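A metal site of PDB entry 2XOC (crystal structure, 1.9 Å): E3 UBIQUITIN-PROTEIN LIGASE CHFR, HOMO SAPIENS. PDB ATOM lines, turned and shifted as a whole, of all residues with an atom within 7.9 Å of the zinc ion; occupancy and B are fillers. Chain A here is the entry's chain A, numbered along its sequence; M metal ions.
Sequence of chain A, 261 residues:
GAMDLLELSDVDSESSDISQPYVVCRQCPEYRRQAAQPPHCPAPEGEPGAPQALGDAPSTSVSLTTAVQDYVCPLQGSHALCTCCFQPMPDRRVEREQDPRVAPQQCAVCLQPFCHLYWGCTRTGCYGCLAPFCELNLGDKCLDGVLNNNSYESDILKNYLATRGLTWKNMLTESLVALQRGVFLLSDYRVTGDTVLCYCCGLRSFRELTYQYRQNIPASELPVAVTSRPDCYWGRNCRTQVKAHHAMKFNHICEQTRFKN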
ATOM      1  N   VAL A  23       5.710 -23.798   2.454  1.00  0.00           N
ATOM      2  CA  VAL A  23       6.411 -23.416   1.231  1.00  0.00           C
ATOM      3  C   VAL A  23       6.272 -21.923   0.927  1.00  0.00           C
ATOM      4  O   VAL A  23       5.163 -21.400   0.861  1.00  0.00           O
ATOM      5  CB  VAL A  23       5.933 -24.242   0.020  1.00  0.00           C
ATOM      6  CG1 VAL A  23       6.548 -23.694  -1.266  1.00  0.00           C
ATOM      7  CG2 VAL A  23       6.292 -25.698   0.204  1.00  0.00           C
ATOM      8  N   VAL A  24       7.407 -21.244   0.765  1.00  0.00           N
ATOM      9  CA  VAL A  24       7.423 -19.830   0.400  1.00  0.00           C
ATOM     10  C   VAL A  24       8.076 -19.669  -0.957  1.00  0.00           C
ATOM     11  O   VAL A  24       9.245 -20.024  -1.134  1.00  0.00           O
ATOM     12  CB  VAL A  24       8.199 -18.991   1.432  1.00  0.00           C
ATOM     13  CG1 VAL A  24       8.195 -17.528   1.037  1.00  0.00           C
ATOM     14  CG2 VAL A  24       7.600 -19.173   2.811  1.00  0.00           C
ATOM     15  N   CYS A  25       7.339 -19.140  -1.932  1.00  0.00           N
ATOM     16  CA  CYS A  25       7.895 -18.965  -3.265  1.00  0.00           C
ATOM     17  C   CYS A  25       8.043 -17.488  -3.621  1.00  0.00           C
ATOM     18  O   CYS A  25       7.611 -16.605  -2.877  1.00  0.00           O
ATOM     19  CB  CYS A  25       7.049 -19.690  -4.321  1.00  0.00           C
ATOM     20  SG  CYS A  25       5.687 -18.712  -4.986  1.00  0.00           S
ATOM     21  N   ARG A  26       8.660 -17.230  -4.777  1.00  0.00           N
ATOM     22  CA  ARG A  26       8.879 -15.863  -5.249  1.00  0.00           C
ATOM     23  C   ARG A  26       7.646 -14.974  -5.096  1.00  0.00           C
ATOM     24  O   ARG A  26       7.766 -13.788  -4.807  1.00  0.00           O
ATOM     25  CB  ARG A  26       9.302 -15.871  -6.726  1.00  0.00           C
ATOM     26  CG  ARG A  26      10.792 -16.023  -6.960  1.00  0.00           C
ATOM     27  CD  ARG A  26      11.109 -15.849  -8.445  1.00  0.00           C
ATOM     28  NE  ARG A  26      11.921 -16.955  -8.953  1.00  0.00           N
ATOM     29  CZ  ARG A  26      12.265 -17.108 -10.236  1.00  0.00           C
ATOM     30  NH1 ARG A  26      11.874 -16.218 -11.132  1.00  0.00           N
ATOM     31  NH2 ARG A  26      13.000 -18.147 -10.610  1.00  0.00           N
ATOM     32  N   GLN A  27       6.464 -15.548  -5.290  1.00  0.00           N
ATOM     33  CA  GLN A  27       5.239 -14.766  -5.344  1.00  0.00           C
ATOM     34  C   GLN A  27       4.353 -14.922  -4.110  1.00  0.00           C
ATOM     35  O   GLN A  27       3.227 -14.433  -4.078  1.00  0.00           O
ATOM     36  CB  GLN A  27       4.448 -15.092  -6.617  1.00  0.00           C
ATOM     37  CG  GLN A  27       5.163 -14.659  -7.899  1.00  0.00           C
ATOM     38  CD  GLN A  27       4.360 -14.949  -9.142  1.00  0.00           C
ATOM     39  OE1 GLN A  27       3.479 -15.802  -9.138  1.00  0.00           O
ATOM     40  NE2 GLN A  27       4.680 -14.255 -10.230  1.00  0.00           N
ATOM     41  N   CYS A  28       4.876 -15.597  -3.085  1.00  0.00           N
ATOM     42  CA  CYS A  28       4.178 -15.719  -1.809  1.00  0.00           C
ATOM     43  C   CYS A  28       4.093 -14.359  -1.113  1.00  0.00           C
ATOM     44  O   CYS A  28       4.968 -13.506  -1.310  1.00  0.00           O
ATOM     45  CB  CYS A  28       4.890 -16.713  -0.895  1.00  0.00           C
ATOM     46  SG  CYS A  28       4.257 -18.398  -0.972  1.00  0.00           S
ATOM     47  N   PRO A  29       3.049 -14.162  -0.295  1.00  0.00           N
ATOM     48  CA  PRO A  29       2.851 -12.930   0.476  1.00  0.00           C
ATOM     49  C   PRO A  29       3.854 -12.827   1.623  1.00  0.00           C
ATOM     50  O   PRO A  29       4.274 -13.858   2.157  1.00  0.00           O
ATOM     51  CB  PRO A  29       1.442 -13.093   1.027  1.00  0.00           C
ATOM     52  CG  PRO A  29       1.273 -14.577   1.146  1.00  0.00           C
ATOM     53  CD  PRO A  29       1.969 -15.135  -0.058  1.00  0.00           C
ATOM     54  N   ARG A  32       3.420 -14.827   4.947  1.00  0.00           N
ATOM     55  CA  ARG A  32       3.838 -16.228   4.875  1.00  0.00           C
ATOM     56  C   ARG A  32       5.340 -16.328   5.089  1.00  0.00           C
ATOM     57  O   ARG A  32       5.836 -17.180   5.817  1.00  0.00           O
ATOM     58  CB  ARG A  32       3.460 -16.824   3.522  1.00  0.00           C
ATOM     59  CG  ARG A  32       1.979 -17.116   3.344  1.00  0.00           C
ATOM     60  CD  ARG A  32       1.657 -18.559   3.701  1.00  0.00           C
ATOM     61  NE  ARG A  32       2.309 -19.497   2.784  1.00  0.00           N
ATOM     62  CZ  ARG A  32       2.218 -20.815   2.893  1.00  0.00           C
ATOM     63  NH1 ARG A  32       1.513 -21.364   3.871  1.00  0.00           N
ATOM     64  NH2 ARG A  32       2.842 -21.593   2.014  1.00  0.00           N
ATOM     65  N   TYR A  71       1.269 -11.512  -9.698  1.00  0.00           N
ATOM     66  CA  TYR A  71       0.521 -12.552  -8.987  1.00  0.00           C
ATOM     67  C   TYR A  71       0.963 -12.674  -7.540  1.00  0.00           C
ATOM     68  O   TYR A  71       2.153 -12.569  -7.224  1.00  0.00           O
ATOM     69  CB  TYR A  71       0.668 -13.901  -9.705  1.00  0.00           C
ATOM     70  CG  TYR A  71      -0.224 -15.001  -9.174  1.00  0.00           C
ATOM     71  CD1 TYR A  71       0.276 -15.969  -8.305  1.00  0.00           C
ATOM     72  CD2 TYR A  71      -1.555 -15.085  -9.535  1.00  0.00           C
ATOM     73  CE1 TYR A  71      -0.527 -16.986  -7.817  1.00  0.00           C
ATOM     74  CE2 TYR A  71      -2.371 -16.089  -9.060  1.00  0.00           C
ATOM     75  CZ  TYR A  71      -1.855 -17.035  -8.199  1.00  0.00           C
ATOM     76  OH  TYR A  71      -2.662 -18.044  -7.722  1.00  0.00           O
ATOM     77  N   VAL A  72      -0.003 -12.898  -6.654  1.00  0.00           N
ATOM     78  CA  VAL A  72       0.283 -13.187  -5.251  1.00  0.00           C
ATOM     79  C   VAL A  72      -0.475 -14.435  -4.838  1.00  0.00           C
ATOM     80  O   VAL A  72      -1.679 -14.550  -5.058  1.00  0.00           O
ATOM     81  CB  VAL A  72      -0.126 -12.022  -4.331  1.00  0.00           C
ATOM     82  CG1 VAL A  72       0.047 -12.429  -2.874  1.00  0.00           C
ATOM     83  CG2 VAL A  72       0.703 -10.783  -4.650  1.00  0.00           C
ATOM     84  N   CYS A  73       0.242 -15.372  -4.232  1.00  0.00           N
ATOM     85  CA  CYS A  73      -0.341 -16.668  -3.884  1.00  0.00           C
ATOM     86  C   CYS A  73      -1.476 -16.569  -2.863  1.00  0.00           C
ATOM     87  O   CYS A  73      -1.303 -15.991  -1.791  1.00  0.00           O
ATOM     88  CB  CYS A  73       0.741 -17.622  -3.384  1.00  0.00           C
ATOM     89  SG  CYS A  73       2.020 -17.944  -4.613  1.00  0.00           S
ATOM     90  N   PRO A  74      -2.648 -17.134  -3.214  1.00  0.00           N
ATOM     91  CA  PRO A  74      -3.816 -17.219  -2.343  1.00  0.00           C
ATOM     92  C   PRO A  74      -3.695 -18.374  -1.360  1.00  0.00           C
ATOM     93  O   PRO A  74      -2.869 -19.263  -1.565  1.00  0.00           O
ATOM     94  CB  PRO A  74      -4.948 -17.489  -3.331  1.00  0.00           C
ATOM     95  CG  PRO A  74      -4.298 -18.261  -4.418  1.00  0.00           C
ATOM     96  CD  PRO A  74      -2.910 -17.689  -4.552  1.00  0.00           C
ATOM     97  N   GLY A  77      -4.550 -21.853  -2.771  1.00  0.00           N
ATOM     98  CA  GLY A  77      -3.705 -22.203  -3.911  1.00  0.00           C
ATOM     99  C   GLY A  77      -2.640 -23.198  -3.504  1.00  0.00           C
ATOM    100  O   GLY A  77      -2.456 -23.473  -2.316  1.00  0.00           O
ATOM    101  N   SER A  78      -1.939 -23.743  -4.489  1.00  0.00           N
ATOM    102  CA  SER A  78      -0.875 -24.713  -4.216  1.00  0.00           C
ATOM    103  C   SER A  78       0.401 -24.332  -4.956  1.00  0.00           C
ATOM    104  O   SER A  78       0.399 -23.407  -5.763  1.00  0.00           O
ATOM    105  CB  SER A  78      -1.328 -26.115  -4.612  1.00  0.00           C
ATOM    106  OG  SER A  78      -1.659 -26.173  -5.988  1.00  0.00           O
ATOM    107  N   HIS A  79       1.474 -25.063  -4.683  1.00  0.00           N
ATOM    108  CA  HIS A  79       2.739 -24.858  -5.380  1.00  0.00           C
ATOM    109  C   HIS A  79       3.188 -26.135  -6.080  1.00  0.00           C
ATOM    110  O   HIS A  79       2.869 -27.245  -5.647  1.00  0.00           O
ATOM    111  CB  HIS A  79       3.830 -24.387  -4.419  1.00  0.00           C
ATOM    112  CG  HIS A  79       3.507 -23.101  -3.720  1.00  0.00           C
ATOM    113  ND1 HIS A  79       2.846 -23.055  -2.512  1.00  0.00           N
ATOM    114  CD2 HIS A  79       3.774 -21.818  -4.053  1.00  0.00           C
ATOM    115  CE1 HIS A  79       2.702 -21.797  -2.140  1.00  0.00           C
ATOM    116  NE2 HIS A  79       3.260 -21.029  -3.053  1.00  0.00           N
ATOM    117  N   PRO A  88       9.928 -23.839  -5.847  1.00  0.00           N
ATOM    118  CA  PRO A  88       8.466 -23.851  -5.911  1.00  0.00           C
ATOM    119  C   PRO A  88       7.916 -22.654  -6.697  1.00  0.00           C
ATOM    120  O   PRO A  88       8.479 -21.559  -6.662  1.00  0.00           O
ATOM    121  CB  PRO A  88       8.055 -23.746  -4.444  1.00  0.00           C
ATOM    122  CG  PRO A  88       9.157 -22.961  -3.823  1.00  0.00           C
ATOM    123  CD  PRO A  88      10.420 -23.402  -4.533  1.00  0.00           C
ATOM    124  N   MET A  89       6.825 -22.899  -7.407  1.00  0.00           N
ATOM    125  CA  MET A  89       6.082 -21.841  -8.081  1.00  0.00           C
ATOM    126  C   MET A  89       4.612 -22.111  -7.821  1.00  0.00           C
ATOM    127  O   MET A  89       4.237 -23.247  -7.521  1.00  0.00           O
ATOM    128  CB  MET A  89       6.363 -21.854  -9.575  1.00  0.00           C
ATOM    129  CG  MET A  89       5.989 -23.159 -10.251  1.00  0.00           C
ATOM    130  SD  MET A  89       6.400 -23.204 -12.006  1.00  0.00           S
ATOM    131  CE  MET A  89       5.925 -24.878 -12.420  1.00  0.00           C
ATOM    132  N   PRO A  90       3.768 -21.068  -7.905  1.00  0.00           N
ATOM    133  CA  PRO A  90       2.333 -21.319  -7.750  1.00  0.00           C
ATOM    134  C   PRO A  90       1.854 -22.224  -8.882  1.00  0.00           C
ATOM    135  O   PRO A  90       2.235 -22.010 -10.024  1.00  0.00           O
ATOM    136  CB  PRO A  90       1.726 -19.920  -7.910  1.00  0.00           C
ATOM    137  CG  PRO A  90       2.736 -19.166  -8.716  1.00  0.00           C
ATOM    138  CD  PRO A  90       4.053 -19.667  -8.225  1.00  0.00           C
ATOM    139  N   ASP A  91       1.044 -23.222  -8.556  1.00  0.00           N
ATOM    140  CA  ASP A  91       0.550 -24.147  -9.572  1.00  0.00           C
ATOM    141  C   ASP A  91      -0.747 -23.639 -10.180  1.00  0.00           C
ATOM    142  O   ASP A  91      -1.822 -23.852  -9.631  1.00  0.00           O
ATOM    143  CB  ASP A  91       0.363 -25.546  -8.999  1.00  0.00           C
ATOM    144  CG  ASP A  91       0.020 -26.569 -10.060  1.00  0.00           C
ATOM    145  OD1 ASP A  91       0.118 -27.778  -9.780  1.00  0.00           O
ATOM    146  OD2 ASP A  91      -0.348 -26.157 -11.184  1.00  0.00           O
ATOM    147  N   TRP A 119       8.164 -17.459 -14.959  1.00  0.00           N
ATOM    148  CA  TRP A 119       8.871 -16.340 -14.344  1.00  0.00           C
ATOM    149  C   TRP A 119      10.391 -16.361 -14.508  1.00  0.00           C
ATOM    150  O   TRP A 119      11.098 -15.590 -13.853  1.00  0.00           O
ATOM    151  CB  TRP A 119       8.497 -16.185 -12.864  1.00  0.00           C
ATOM    152  CG  TRP A 119       8.868 -17.347 -11.986  1.00  0.00           C
ATOM    153  CD1 TRP A 119       9.772 -18.322 -12.249  1.00  0.00           C
ATOM    154  CD2 TRP A 119       8.347 -17.620 -10.677  1.00  0.00           C
ATOM    155  NE1 TRP A 119       9.837 -19.203 -11.193  1.00  0.00           N
ATOM    156  CE2 TRP A 119       8.976 -18.791 -10.220  1.00  0.00           C
ATOM    157  CE3 TRP A 119       7.396 -17.001  -9.861  1.00  0.00           C
ATOM    158  CZ2 TRP A 119       8.692 -19.355  -8.975  1.00  0.00           C
ATOM    159  CZ3 TRP A 119       7.120 -17.554  -8.620  1.00  0.00           C
ATOM    160  CH2 TRP A 119       7.762 -18.717  -8.187  1.00  0.00           C
HETATM  161 ZN    ZN M   1       3.875 -18.913  -3.422  1.00  0.00          ZN
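The side-chain sulfur of Cys 25 sits close to the backbone NH of Gln 27 (3.3 Å). The backbone NH of Cys 73 is in hydrogen-bond range of the backbone carbonyl oxygen of Gln 27 (3.1 Å). The backbone carbonyl oxygen (O) of Val 23 lies close to the side-chain sulfur (SG) of Cys 28, 3.6 Å away.
The nearest printed residue that does not touch the zinc ion is Gln 27 (4.1 Å).
The zinc ion is bound by NE2 of His 79, SG of Cys 25, SG of Cys 73 and SG of Cys 28.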
